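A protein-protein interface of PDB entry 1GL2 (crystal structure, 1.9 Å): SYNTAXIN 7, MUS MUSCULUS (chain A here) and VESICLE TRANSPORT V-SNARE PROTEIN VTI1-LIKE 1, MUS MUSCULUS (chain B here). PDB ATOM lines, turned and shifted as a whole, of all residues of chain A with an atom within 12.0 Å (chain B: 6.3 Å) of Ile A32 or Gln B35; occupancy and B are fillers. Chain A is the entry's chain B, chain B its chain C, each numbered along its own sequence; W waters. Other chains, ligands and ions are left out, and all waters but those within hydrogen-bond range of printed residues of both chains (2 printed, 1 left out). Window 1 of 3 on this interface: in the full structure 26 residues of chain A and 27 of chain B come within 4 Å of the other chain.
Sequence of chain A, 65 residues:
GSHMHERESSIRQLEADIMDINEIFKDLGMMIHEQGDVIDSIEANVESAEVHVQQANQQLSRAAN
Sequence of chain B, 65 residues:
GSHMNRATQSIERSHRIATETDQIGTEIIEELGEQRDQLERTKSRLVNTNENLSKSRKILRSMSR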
ATOM      1  N   ASN A  22     -18.436 -23.980 -16.879  1.00  0.00           N
ATOM      2  CA  ASN A  22     -17.970 -22.929 -15.983  1.00  0.00           C
ATOM      3  C   ASN A  22     -19.068 -22.600 -14.966  1.00  0.00           C
ATOM      4  O   ASN A  22     -18.793 -22.405 -13.782  1.00  0.00           O
ATOM      5  CB  ASN A  22     -17.601 -21.684 -16.792  1.00  0.00           C
ATOM      6  CG  ASN A  22     -17.242 -20.503 -15.917  1.00  0.00           C
ATOM      7  OD1 ASN A  22     -18.068 -19.619 -15.673  1.00  0.00           O
ATOM      8  ND2 ASN A  22     -16.001 -20.483 -15.430  1.00  0.00           N
ATOM      9  N   GLU A  23     -20.314 -22.541 -15.430  1.00  0.00           N
ATOM     10  CA  GLU A  23     -21.432 -22.253 -14.540  1.00  0.00           C
ATOM     11  C   GLU A  23     -21.693 -23.401 -13.561  1.00  0.00           C
ATOM     12  O   GLU A  23     -22.173 -23.173 -12.455  1.00  0.00           O
ATOM     13  CB  GLU A  23     -22.699 -21.962 -15.345  1.00  0.00           C
ATOM     14  CG  GLU A  23     -22.679 -20.636 -16.098  1.00  0.00           C
ATOM     15  CD  GLU A  23     -22.426 -19.435 -15.190  1.00  0.00           C
ATOM     16  OE1 GLU A  23     -22.982 -19.389 -14.068  1.00  0.00           O
ATOM     17  OE2 GLU A  23     -21.677 -18.524 -15.605  1.00  0.00           O
ATOM     18  N   ILE A  24     -21.384 -24.633 -13.957  1.00  0.00           N
ATOM     19  CA  ILE A  24     -21.591 -25.769 -13.062  1.00  0.00           C
ATOM     20  C   ILE A  24     -20.584 -25.677 -11.916  1.00  0.00           C
ATOM     21  O   ILE A  24     -20.923 -25.914 -10.755  1.00  0.00           O
ATOM     22  CB  ILE A  24     -21.397 -27.123 -13.797  1.00  0.00           C
ATOM     23  CG1 ILE A  24     -22.453 -27.278 -14.897  1.00  0.00           C
ATOM     24  CG2 ILE A  24     -21.490 -28.277 -12.805  1.00  0.00           C
ATOM     25  CD1 ILE A  24     -22.296 -28.546 -15.730  1.00  0.00           C
ATOM     26  N   PHE A  25     -19.343 -25.332 -12.251  1.00  0.00           N
ATOM     27  CA  PHE A  25     -18.301 -25.191 -11.242  1.00  0.00           C
ATOM     28  C   PHE A  25     -18.705 -24.102 -10.264  1.00  0.00           C
ATOM     29  O   PHE A  25     -18.568 -24.269  -9.052  1.00  0.00           O
ATOM     30  CB  PHE A  25     -16.954 -24.815 -11.873  1.00  0.00           C
ATOM     31  CG  PHE A  25     -16.079 -25.995 -12.212  1.00  0.00           C
ATOM     32  CD1 PHE A  25     -16.331 -26.770 -13.337  1.00  0.00           C
ATOM     33  CD2 PHE A  25     -14.983 -26.316 -11.407  1.00  0.00           C
ATOM     34  CE1 PHE A  25     -15.502 -27.848 -13.661  1.00  0.00           C
ATOM     35  CE2 PHE A  25     -14.150 -27.392 -11.721  1.00  0.00           C
ATOM     36  CZ  PHE A  25     -14.409 -28.157 -12.850  1.00  0.00           C
ATOM     37  N   LYS A  26     -19.204 -22.986 -10.794  1.00  0.00           N
ATOM     38  CA  LYS A  26     -19.623 -21.871  -9.956  1.00  0.00           C
ATOM     39  C   LYS A  26     -20.778 -22.265  -9.054  1.00  0.00           C
ATOM     40  O   LYS A  26     -20.825 -21.873  -7.890  1.00  0.00           O
ATOM     41  CB  LYS A  26     -20.019 -20.671 -10.815  1.00  0.00           C
ATOM     42  CG  LYS A  26     -18.825 -19.926 -11.390  1.00  0.00           C
ATOM     43  CD  LYS A  26     -19.253 -18.796 -12.307  1.00  0.00           C
ATOM     44  CE  LYS A  26     -18.034 -18.128 -12.906  1.00  0.00           C
ATOM     45  NZ  LYS A  26     -18.394 -17.164 -13.981  1.00  0.00           N
ATOM     46  N   ASP A  27     -21.705 -23.048  -9.596  1.00  0.00           N
ATOM     47  CA  ASP A  27     -22.857 -23.516  -8.837  1.00  0.00           C
ATOM     48  C   ASP A  27     -22.372 -24.434  -7.709  1.00  0.00           C
ATOM     49  O   ASP A  27     -22.748 -24.262  -6.548  1.00  0.00           O
ATOM     50  CB  ASP A  27     -23.809 -24.255  -9.777  1.00  0.00           C
ATOM     51  CG  ASP A  27     -25.062 -24.743  -9.080  1.00  0.00           C
ATOM     52  OD1 ASP A  27     -25.581 -24.019  -8.204  1.00  0.00           O
ATOM     53  OD2 ASP A  27     -25.540 -25.845  -9.422  1.00  0.00           O
ATOM     54  N   LEU A  28     -21.527 -25.397  -8.057  1.00  0.00           N
ATOM     55  CA  LEU A  28     -20.970 -26.325  -7.077  1.00  0.00           C
ATOM     56  C   LEU A  28     -20.189 -25.531  -6.036  1.00  0.00           C
ATOM     57  O   LEU A  28     -20.325 -25.755  -4.831  1.00  0.00           O
ATOM     58  CB  LEU A  28     -20.029 -27.327  -7.764  1.00  0.00           C
ATOM     59  CG  LEU A  28     -19.220 -28.269  -6.857  1.00  0.00           C
ATOM     60  CD1 LEU A  28     -20.148 -29.175  -6.075  1.00  0.00           C
ATOM     61  CD2 LEU A  28     -18.264 -29.097  -7.697  1.00  0.00           C
ATOM     62  N   GLY A  29     -19.372 -24.596  -6.510  1.00  0.00           N
ATOM     63  CA  GLY A  29     -18.577 -23.781  -5.610  1.00  0.00           C
ATOM     64  C   GLY A  29     -19.408 -22.977  -4.631  1.00  0.00           C
ATOM     65  O   GLY A  29     -19.072 -22.885  -3.449  1.00  0.00           O
ATOM     66  N   MET A  30     -20.494 -22.386  -5.122  1.00  0.00           N
ATOM     67  CA  MET A  30     -21.373 -21.575  -4.283  1.00  0.00           C
ATOM     68  C   MET A  30     -21.991 -22.399  -3.167  1.00  0.00           C
ATOM     69  O   MET A  30     -22.016 -21.976  -2.018  1.00  0.00           O
ATOM     70  CB  MET A  30     -22.498 -20.958  -5.121  1.00  0.00           C
ATOM     71  CG  MET A  30     -23.501 -20.129  -4.310  1.00  0.00           C
ATOM     72  SD  MET A  30     -24.906 -19.501  -5.303  1.00  0.00           S
ATOM     73  CE  MET A  30     -26.076 -19.000  -4.000  1.00  0.00           C
ATOM     74  N   MET A  31     -22.490 -23.579  -3.502  1.00  0.00           N
ATOM     75  CA  MET A  31     -23.120 -24.414  -2.494  1.00  0.00           C
ATOM     76  C   MET A  31     -22.142 -24.989  -1.482  1.00  0.00           C
ATOM     77  O   MET A  31     -22.482 -25.150  -0.313  1.00  0.00           O
ATOM     78  CB  MET A  31     -23.924 -25.524  -3.167  1.00  0.00           C
ATOM     79  CG  MET A  31     -25.131 -24.990  -3.932  1.00  0.00           C
ATOM     80  SD  MET A  31     -26.179 -26.322  -4.488  1.00  0.00           S
ATOM     81  CE  MET A  31     -25.468 -26.667  -6.096  1.00  0.00           C
ATOM     82  N   ILE A  32     -20.928 -25.300  -1.926  1.00  0.00           N
ATOM     83  CA  ILE A  32     -19.914 -25.822  -1.020  1.00  0.00           C
ATOM     84  C   ILE A  32     -19.592 -24.754   0.022  1.00  0.00           C
ATOM     85  O   ILE A  32     -19.502 -25.040   1.219  1.00  0.00           O
ATOM     86  CB  ILE A  32     -18.636 -26.207  -1.795  1.00  0.00           C
ATOM     87  CG1 ILE A  32     -18.836 -27.581  -2.444  1.00  0.00           C
ATOM     88  CG2 ILE A  32     -17.423 -26.203  -0.868  1.00  0.00           C
ATOM     89  CD1 ILE A  32     -17.724 -27.981  -3.382  1.00  0.00           C
ATOM     90  N   HIS A  33     -19.444 -23.516  -0.440  1.00  0.00           N
ATOM     91  CA  HIS A  33     -19.129 -22.383   0.426  1.00  0.00           C
ATOM     92  C   HIS A  33     -20.245 -22.106   1.445  1.00  0.00           C
ATOM     93  O   HIS A  33     -19.979 -21.906   2.631  1.00  0.00           O
ATOM     94  CB  HIS A  33     -18.885 -21.147  -0.437  1.00  0.00           C
ATOM     95  CG  HIS A  33     -18.311 -19.985   0.310  1.00  0.00           C
ATOM     96  ND1 HIS A  33     -17.119 -20.057   1.003  1.00  0.00           N
ATOM     97  CD2 HIS A  33     -18.750 -18.712   0.452  1.00  0.00           C
ATOM     98  CE1 HIS A  33     -16.851 -18.879   1.539  1.00  0.00           C
ATOM     99  NE2 HIS A  33     -17.824 -18.045   1.219  1.00  0.00           N
ATOM    100  N   GLU A  34     -21.494 -22.096   0.982  1.00  0.00           N
ATOM    101  CA  GLU A  34     -22.620 -21.849   1.873  1.00  0.00           C
ATOM    102  C   GLU A  34     -22.817 -22.982   2.883  1.00  0.00           C
ATOM    103  O   GLU A  34     -23.192 -22.745   4.035  1.00  0.00           O
ATOM    104  CB  GLU A  34     -23.901 -21.637   1.061  1.00  0.00           C
ATOM    105  CG  GLU A  34     -23.918 -20.308   0.314  1.00  0.00           C
ATOM    106  CD  GLU A  34     -25.279 -19.969  -0.282  1.00  0.00           C
ATOM    107  OE1 GLU A  34     -25.388 -18.920  -0.954  1.00  0.00           O
ATOM    108  OE2 GLU A  34     -26.238 -20.746  -0.079  1.00  0.00           O
ATOM    109  N   GLN A  35     -22.564 -24.212   2.452  1.00  0.00           N
ATOM    110  CA  GLN A  35     -22.706 -25.350   3.343  1.00  0.00           C
ATOM    111  C   GLN A  35     -21.652 -25.279   4.430  1.00  0.00           C
ATOM    112  O   GLN A  35     -21.748 -25.980   5.440  1.00  0.00           O
ATOM    113  CB  GLN A  35     -22.601 -26.658   2.564  1.00  0.00           C
ATOM    114  CG  GLN A  35     -23.898 -27.014   1.859  1.00  0.00           C
ATOM    115  CD  GLN A  35     -23.746 -28.192   0.931  1.00  0.00           C
ATOM    116  OE1 GLN A  35     -22.802 -28.972   1.055  1.00  0.00           O
ATOM    117  NE2 GLN A  35     -24.683 -28.340   0.000  1.00  0.00           N
ATOM    118  N   GLY A  36     -20.652 -24.426   4.227  1.00  0.00           N
ATOM    119  CA  GLY A  36     -19.621 -24.249   5.235  1.00  0.00           C
ATOM    120  C   GLY A  36     -20.232 -23.756   6.543  1.00  0.00           C
ATOM    121  O   GLY A  36     -19.742 -24.082   7.627  1.00  0.00           O
ATOM    122  N   ASP A  37     -21.303 -22.968   6.443  1.00  0.00           N
ATOM    123  CA  ASP A  37     -21.989 -22.442   7.626  1.00  0.00           C
ATOM    124  C   ASP A  37     -22.618 -23.576   8.419  1.00  0.00           C
ATOM    125  O   ASP A  37     -22.611 -23.561   9.646  1.00  0.00           O
ATOM    126  CB  ASP A  37     -23.112 -21.471   7.248  1.00  0.00           C
ATOM    127  CG  ASP A  37     -22.611 -20.229   6.550  1.00  0.00           C
ATOM    128  OD1 ASP A  37     -21.391 -19.951   6.610  1.00  0.00           O
ATOM    129  OD2 ASP A  37     -23.452 -19.525   5.948  1.00  0.00           O
ATOM    130  N   VAL A  38     -23.188 -24.543   7.708  1.00  0.00           N
ATOM    131  CA  VAL A  38     -23.829 -25.687   8.345  1.00  0.00           C
ATOM    132  C   VAL A  38     -22.772 -26.490   9.104  1.00  0.00           C
ATOM    133  O   VAL A  38     -22.989 -26.894  10.245  1.00  0.00           O
ATOM    134  CB  VAL A  38     -24.524 -26.577   7.294  1.00  0.00           C
ATOM    135  CG1 VAL A  38     -25.192 -27.761   7.960  1.00  0.00           C
ATOM    136  CG2 VAL A  38     -25.552 -25.755   6.534  1.00  0.00           C
ATOM    137  N   ILE A  39     -21.621 -26.703   8.472  1.00  0.00           N
ATOM    138  CA  ILE A  39     -20.533 -27.443   9.100  1.00  0.00           C
ATOM    139  C   ILE A  39     -20.028 -26.682  10.328  1.00  0.00           C
ATOM    140  O   ILE A  39     -19.706 -27.290  11.349  1.00  0.00           O
ATOM    141  CB  ILE A  39     -19.391 -27.672   8.098  1.00  0.00           C
ATOM    142  CG1 ILE A  39     -19.900 -28.574   6.975  1.00  0.00           C
ATOM    143  CG2 ILE A  39     -18.183 -28.306   8.791  1.00  0.00           C
ATOM    144  CD1 ILE A  39     -18.941 -28.703   5.813  1.00  0.00           C
ATOM    145  N   ASP A  40     -19.974 -25.353  10.229  1.00  0.00           N
ATOM    146  CA  ASP A  40     -19.542 -24.515  11.356  1.00  0.00           C
ATOM    147  C   ASP A  40     -20.464 -24.759  12.557  1.00  0.00           C
ATOM    148  O   ASP A  40     -20.005 -24.868  13.696  1.00  0.00           O
ATOM    149  CB  ASP A  40     -19.597 -23.024  10.982  1.00  0.00           C
ATOM    150  CG  ASP A  40     -18.434 -22.587  10.098  1.00  0.00           C
ATOM    151  OD1 ASP A  40     -18.508 -21.474   9.531  1.00  0.00           O
ATOM    152  OD2 ASP A  40     -17.445 -23.343   9.975  1.00  0.00           O
ATOM    153  N   SER A  41     -21.766 -24.836  12.287  1.00  0.00           N
ATOM    154  CA  SER A  41     -22.772 -25.065  13.319  1.00  0.00           C
ATOM    155  C   SER A  41     -22.655 -26.458  13.914  1.00  0.00           C
ATOM    156  O   SER A  41     -22.839 -26.636  15.118  1.00  0.00           O
ATOM    157  CB  SER A  41     -24.180 -24.892  12.744  1.00  0.00           C
ATOM    158  OG  SER A  41     -24.372 -23.569  12.282  1.00  0.00           O
ATOM    159  N   ILE A  42     -22.368 -27.442  13.066  1.00  0.00           N
ATOM    160  CA  ILE A  42     -22.219 -28.826  13.505  1.00  0.00           C
ATOM    161  C   ILE A  42     -21.040 -28.921  14.465  1.00  0.00           C
ATOM    162  O   ILE A  42     -21.130 -29.522  15.540  1.00  0.00           O
ATOM    163  CB  ILE A  42     -21.979 -29.757  12.298  1.00  0.00           C
ATOM    164  CG1 ILE A  42     -23.277 -29.895  11.503  1.00  0.00           C
ATOM    165  CG2 ILE A  42     -21.459 -31.113  12.757  1.00  0.00           C
ATOM    166  CD1 ILE A  42     -23.121 -30.658  10.210  1.00  0.00           C
ATOM    167  N   GLU A  43     -19.932 -28.312  14.067  1.00  0.00           N
ATOM    168  CA  GLU A  43     -18.739 -28.316  14.884  1.00  0.00           C
ATOM    169  C   GLU A  43     -18.993 -27.623  16.226  1.00  0.00           C
ATOM    170  O   GLU A  43     -18.571 -28.114  17.278  1.00  0.00           O
ATOM    171  CB  GLU A  43     -17.613 -27.615  14.131  1.00  0.00           C
ATOM    172  CG  GLU A  43     -16.336 -27.490  14.924  1.00  0.00           C
ATOM    173  CD  GLU A  43     -15.204 -26.983  14.075  1.00  0.00           C
ATOM    174  OE1 GLU A  43     -15.405 -25.971  13.374  1.00  0.00           O
ATOM    175  OE2 GLU A  43     -14.116 -27.595  14.110  1.00  0.00           O
ATOM    176  N   ALA A  44     -19.695 -26.490  16.178  1.00  0.00           N
ATOM    177  CA  ALA A  44     -20.010 -25.714  17.375  1.00  0.00           C
ATOM    178  C   ALA A  44     -20.898 -26.469  18.361  1.00  0.00           C
ATOM    179  O   ALA A  44     -20.670 -26.415  19.572  1.00  0.00           O
ATOM    180  CB  ALA A  44     -20.679 -24.388  16.985  1.00  0.00           C
ATOM    181  N   GLU A  47     -18.705 -29.117  20.005  1.00  0.00           N
ATOM    182  CA  GLU A  47     -17.743 -28.560  20.955  1.00  0.00           C
ATOM    183  C   GLU A  47     -18.457 -28.155  22.237  1.00  0.00           C
ATOM    184  O   GLU A  47     -17.930 -28.319  23.339  1.00  0.00           O
ATOM    185  CB  GLU A  47     -17.041 -27.338  20.365  1.00  0.00           C
ATOM    186  CG  GLU A  47     -16.051 -27.659  19.271  1.00  0.00           C
ATOM    187  CD  GLU A  47     -15.195 -26.465  18.902  1.00  0.00           C
ATOM    188  OE1 GLU A  47     -14.540 -25.905  19.807  1.00  0.00           O
ATOM    189  OE2 GLU A  47     -15.169 -26.086  17.711  1.00  0.00           O
ATOM    190  N   ILE B  28     -12.230 -24.854  -5.133  1.00  0.00           N
ATOM    191  CA  ILE B  28     -13.192 -25.814  -4.597  1.00  0.00           C
ATOM    192  C   ILE B  28     -12.486 -26.938  -3.856  1.00  0.00           C
ATOM    193  O   ILE B  28     -12.893 -27.326  -2.761  1.00  0.00           O
ATOM    194  CB  ILE B  28     -14.059 -26.442  -5.722  1.00  0.00           C
ATOM    195  CG1 ILE B  28     -15.105 -25.432  -6.202  1.00  0.00           C
ATOM    196  CG2 ILE B  28     -14.741 -27.728  -5.218  1.00  0.00           C
ATOM    197  CD1 ILE B  28     -15.928 -25.911  -7.391  1.00  0.00           C
ATOM    198  N   GLU B  30      -9.542 -26.892  -2.481  1.00  0.00           N
ATOM    199  CA  GLU B  30      -8.941 -26.377  -1.257  1.00  0.00           C
ATOM    200  C   GLU B  30      -9.992 -26.208  -0.164  1.00  0.00           C
ATOM    201  O   GLU B  30      -9.761 -26.555   0.996  1.00  0.00           O
ATOM    202  CB  GLU B  30      -8.253 -25.029  -1.526  1.00  0.00           C
ATOM    203  CG  GLU B  30      -7.407 -24.505  -0.361  1.00  0.00           C
ATOM    204  CD  GLU B  30      -8.240 -23.980   0.799  1.00  0.00           C
ATOM    205  OE1 GLU B  30      -7.785 -24.107   1.958  1.00  0.00           O
ATOM    206  OE2 GLU B  30      -9.338 -23.427   0.558  1.00  0.00           O
ATOM    207  N   GLU B  31     -11.149 -25.677  -0.536  1.00  0.00           N
ATOM    208  CA  GLU B  31     -12.203 -25.457   0.438  1.00  0.00           C
ATOM    209  C   GLU B  31     -12.759 -26.774   0.970  1.00  0.00           C
ATOM    210  O   GLU B  31     -13.074 -26.874   2.150  1.00  0.00           O
ATOM    211  CB  GLU B  31     -13.314 -24.585  -0.162  1.00  0.00           C
ATOM    212  CG  GLU B  31     -14.389 -24.199   0.849  1.00  0.00           C
ATOM    213  CD  GLU B  31     -15.218 -22.999   0.419  1.00  0.00           C
ATOM    214  OE1 GLU B  31     -15.515 -22.866  -0.788  1.00  0.00           O
ATOM    215  OE2 GLU B  31     -15.590 -22.191   1.292  1.00  0.00           O
ATOM    216  N   LEU B  32     -12.869 -27.790   0.120  1.00  0.00           N
ATOM    217  CA  LEU B  32     -13.364 -29.079   0.590  1.00  0.00           C
ATOM    218  C   LEU B  32     -12.344 -29.694   1.553  1.00  0.00           C
ATOM    219  O   LEU B  32     -12.695 -30.458   2.459  1.00  0.00           O
ATOM    220  CB  LEU B  32     -13.613 -30.033  -0.584  1.00  0.00           C
ATOM    221  CG  LEU B  32     -14.826 -29.724  -1.471  1.00  0.00           C
ATOM    222  CD1 LEU B  32     -14.927 -30.781  -2.561  1.00  0.00           C
ATOM    223  CD2 LEU B  32     -16.092 -29.711  -0.640  1.00  0.00           C
ATOM    224  N   GLY B  33     -11.077 -29.357   1.357  1.00  0.00           N
ATOM    225  CA  GLY B  33     -10.051 -29.878   2.238  1.00  0.00           C
ATOM    226  C   GLY B  33     -10.225 -29.314   3.642  1.00  0.00           C
ATOM    227  O   GLY B  33     -10.094 -30.042   4.630  1.00  0.00           O
ATOM    228  N   GLU B  34     -10.520 -28.020   3.733  1.00  0.00           N
ATOM    229  CA  GLU B  34     -10.724 -27.380   5.028  1.00  0.00           C
ATOM    230  C   GLU B  34     -11.960 -27.958   5.708  1.00  0.00           C
ATOM    231  O   GLU B  34     -11.974 -28.186   6.922  1.00  0.00           O
ATOM    232  CB  GLU B  34     -10.913 -25.869   4.862  1.00  0.00           C
ATOM    233  CG  GLU B  34      -9.734 -25.141   4.220  1.00  0.00           C
ATOM    234  CD  GLU B  34      -9.882 -23.621   4.263  1.00  0.00           C
ATOM    235  OE1 GLU B  34     -10.941 -23.127   4.709  1.00  0.00           O
ATOM    236  OE2 GLU B  34      -8.937 -22.921   3.844  1.00  0.00           O
ATOM    237  N   GLN B  35     -13.002 -28.191   4.919  1.00  0.00           N
ATOM    238  CA  GLN B  35     -14.244 -28.730   5.456  1.00  0.00           C
ATOM    239  C   GLN B  35     -14.079 -30.172   5.930  1.00  0.00           C
ATOM    240  O   GLN B  35     -14.648 -30.560   6.953  1.00  0.00           O
ATOM    241  CB  GLN B  35     -15.360 -28.596   4.413  1.00  0.00           C
ATOM    242  CG  GLN B  35     -15.658 -27.130   4.074  1.00  0.00           C
ATOM    243  CD  GLN B  35     -16.857 -26.956   3.157  1.00  0.00           C
ATOM    244  OE1 GLN B  35     -17.363 -27.920   2.587  1.00  0.00           O
ATOM    245  NE2 GLN B  35     -17.309 -25.717   3.006  1.00  0.00           N
ATOM    246  N   ARG B  36     -13.299 -30.964   5.198  1.00  0.00           N
ATOM    247  CA  ARG B  36     -13.046 -32.342   5.597  1.00  0.00           C
ATOM    248  C   ARG B  36     -12.377 -32.341   6.969  1.00  0.00           C
ATOM    249  O   ARG B  36     -12.797 -33.068   7.861  1.00  0.00           O
ATOM    250  CB  ARG B  36     -12.122 -33.049   4.598  1.00  0.00           C
ATOM    251  CG  ARG B  36     -11.478 -34.316   5.169  1.00  0.00           C
ATOM    252  CD  ARG B  36     -10.388 -34.876   4.265  1.00  0.00           C
ATOM    253  NE  ARG B  36     -10.930 -35.802   3.274  1.00  0.00           N
ATOM    254  CZ  ARG B  36     -11.239 -37.070   3.525  1.00  0.00           C
ATOM    255  NH1 ARG B  36     -11.052 -37.574   4.737  1.00  0.00           N
ATOM    256  NH2 ARG B  36     -11.745 -37.831   2.566  1.00  0.00           N
ATOM    257  N   ASP B  37     -11.337 -31.522   7.126  1.00  0.00           N
ATOM    258  CA  ASP B  37     -10.596 -31.432   8.388  1.00  0.00           C
ATOM    259  C   ASP B  37     -11.496 -30.993   9.539  1.00  0.00           C
ATOM    260  O   ASP B  37     -11.356 -31.461  10.672  1.00  0.00           O
ATOM    261  CB  ASP B  37      -9.421 -30.448   8.267  1.00  0.00           C
ATOM    262  CG  ASP B  37      -8.336 -30.945   7.331  1.00  0.00           C
ATOM    263  OD1 ASP B  37      -8.274 -32.171   7.087  1.00  0.00           O
ATOM    264  OD2 ASP B  37      -7.536 -30.111   6.852  1.00  0.00           O
ATOM    265  N   GLN B  38     -12.412 -30.082   9.235  1.00  0.00           N
ATOM    266  CA  GLN B  38     -13.351 -29.573  10.216  1.00  0.00           C
ATOM    267  C   GLN B  38     -14.258 -30.719  10.692  1.00  0.00           C
ATOM    268  O   GLN B  38     -14.540 -30.852  11.886  1.00  0.00           O
ATOM    269  CB  GLN B  38     -14.158 -28.447   9.571  1.00  0.00           C
ATOM    270  CG  GLN B  38     -15.071 -27.686  10.498  1.00  0.00           C
ATOM    271  CD  GLN B  38     -15.491 -26.354   9.907  1.00  0.00           C
ATOM    272  OE1 GLN B  38     -15.321 -26.109   8.708  1.00  0.00           O
ATOM    273  NE2 GLN B  38     -16.048 -25.489  10.742  1.00  0.00           N
ATOM    274  N   LEU B  39     -14.702 -31.552   9.754  1.00  0.00           N
ATOM    275  CA  LEU B  39     -15.547 -32.694  10.084  1.00  0.00           C
ATOM    276  C   LEU B  39     -14.753 -33.733  10.881  1.00  0.00           C
ATOM    277  O   LEU B  39     -15.295 -34.396  11.763  1.00  0.00           O
ATOM    278  CB  LEU B  39     -16.113 -33.330   8.810  1.00  0.00           C
ATOM    279  CG  LEU B  39     -17.176 -32.550   8.023  1.00  0.00           C
ATOM    280  CD1 LEU B  39     -17.445 -33.278   6.711  1.00  0.00           C
ATOM    281  CD2 LEU B  39     -18.470 -32.421   8.823  1.00  0.00           C
ATOM    282  N   GLU B  40     -13.466 -33.874  10.580  1.00  0.00           N
ATOM    283  CA  GLU B  40     -12.632 -34.834  11.303  1.00  0.00           C
ATOM    284  C   GLU B  40     -12.369 -34.343  12.729  1.00  0.00           C
ATOM    285  O   GLU B  40     -12.356 -35.135  13.676  1.00  0.00           O
ATOM    286  CB  GLU B  40     -11.304 -35.063  10.573  1.00  0.00           C
ATOM    287  CG  GLU B  40     -11.432 -35.710   9.194  1.00  0.00           C
ATOM    288  CD  GLU B  40     -12.048 -37.101   9.219  1.00  0.00           C
ATOM    289  OE1 GLU B  40     -12.125 -37.729   8.146  1.00  0.00           O
ATOM    290  OE2 GLU B  40     -12.455 -37.574  10.297  1.00  0.00           O
HETATM  291  O   HOH W   1     -16.238 -23.324  -3.072  1.00  0.00           O
HETATM  292  O   HOH W   2     -15.254 -22.775   8.788  1.00  0.00           O
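The side-chain carboxylate of Glu A43 lies within hydrogen-bond range of the side-chain amide nitrogen of Gln B38, 2.8 Å away. The side-chain carboxylate of Asp A40 sits at hydrogen-bond distance from the side-chain amide nitrogen of Gln B38, 2.7 Å away. The side-chain amide nitrogen (NE2) of Gln B35 sits at hydrogen-bond distance from the backbone carbonyl oxygen (O) of Ile A32. The side-chain carboxylate (OE2) of Glu B31 is in hydrogen-bond range of a ring nitrogen (ND1) of His A33, 2.6 Å away.
Among the printed residues, pairs that only touch across the chains: Ile A39 with Gln B38 (3.5 Å), Ile A32 with Ile B28 (3.5 Å), Phe A25 with Ile B28 (3.5 Å), Gly A36 with Gln B35 (3.5 Å), Ile A32 with Leu B32 (3.6 Å), Ile A39 with Gln B35 (3.7 Å), Gly A29 with Ile B28 (3.8 Å), Ile A32 with Glu B31 (3.8 Å) and Leu A28 with Ile B28 (3.96 Å).
Ile A32 touches just these residues of chain B: Ile B28, Glu B31, Leu B32 and Gln B35. Gln B35 touches just these residues of chain A: Ile A32 (2.9 Å), Gly A36 (3.5 Å) and Ile A39 (3.7 Å). Ile B28 touches just these residues of chain A: Phe A25, Leu A28, Gly A29 and Ile A32. Glu B31 touches just these residues of chain A: Ile A32 and His A33. Leu B32 touches just one residue of chain A: Ile A32. No residue of chain A comes within 4 Å of Gly B33. No residue of chain A comes within 4 Å of Glu B34. No residue of chain A comes within 4 Å of Asp B37. Gln B38 touches three residues of chain A. Of the printed residues of chain B, Phe A25 touches Ile B28. Printed residues of chain B within 4 Å of Glu A43: Gln B38. Of the printed residues of chain B, Gly A36 touches Gln B35 (3.5 Å). Of the printed residues of chain B, Gly A29 touches Ile B28 (3.8 Å). Val A38 touches none of the printed residues of chain B. Glu A47 touches none of the printed residues of chain B. The nearest printed residue of chain B that does not touch Ile A32 is Gly B33 (7.4 Å). The nearest printed residue of chain B that does not touch His A33 is Gln B35 (4.6 Å).
Printed residues of chain A that touch a printed residue of chain B: Phe A25, Leu A28, Gly A29, Ile A32, His A33, Gly A36, Ile A39, Asp A40 and Glu A43. Hydrophobic or aromatic side chains of chain A within 4 Å of the printed part of chain B: Leu A28, Ile A32, His A33 and Ile A39. Printed residues of chain B that touch a printed residue of chain A: Ile B28, Glu B31, Leu B32, Gln B35 and Gln B38. Hydrophobic or aromatic side chains of chain B within 4 Å of the printed part of chain A: Ile B28 and Leu B32. Among the printed residues, 13 pairs touch across the chains.
Water W1 lies within hydrogen-bond range of the side-chain carboxylate of Glu B31 (2.4 Å) and the backbone carbonyl oxygen of Gly A29 (2.9 Å). Water W2 bridges OD2 of Asp A40 (2.6 Å) and OE1 of Gln B38 (3.3 Å).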
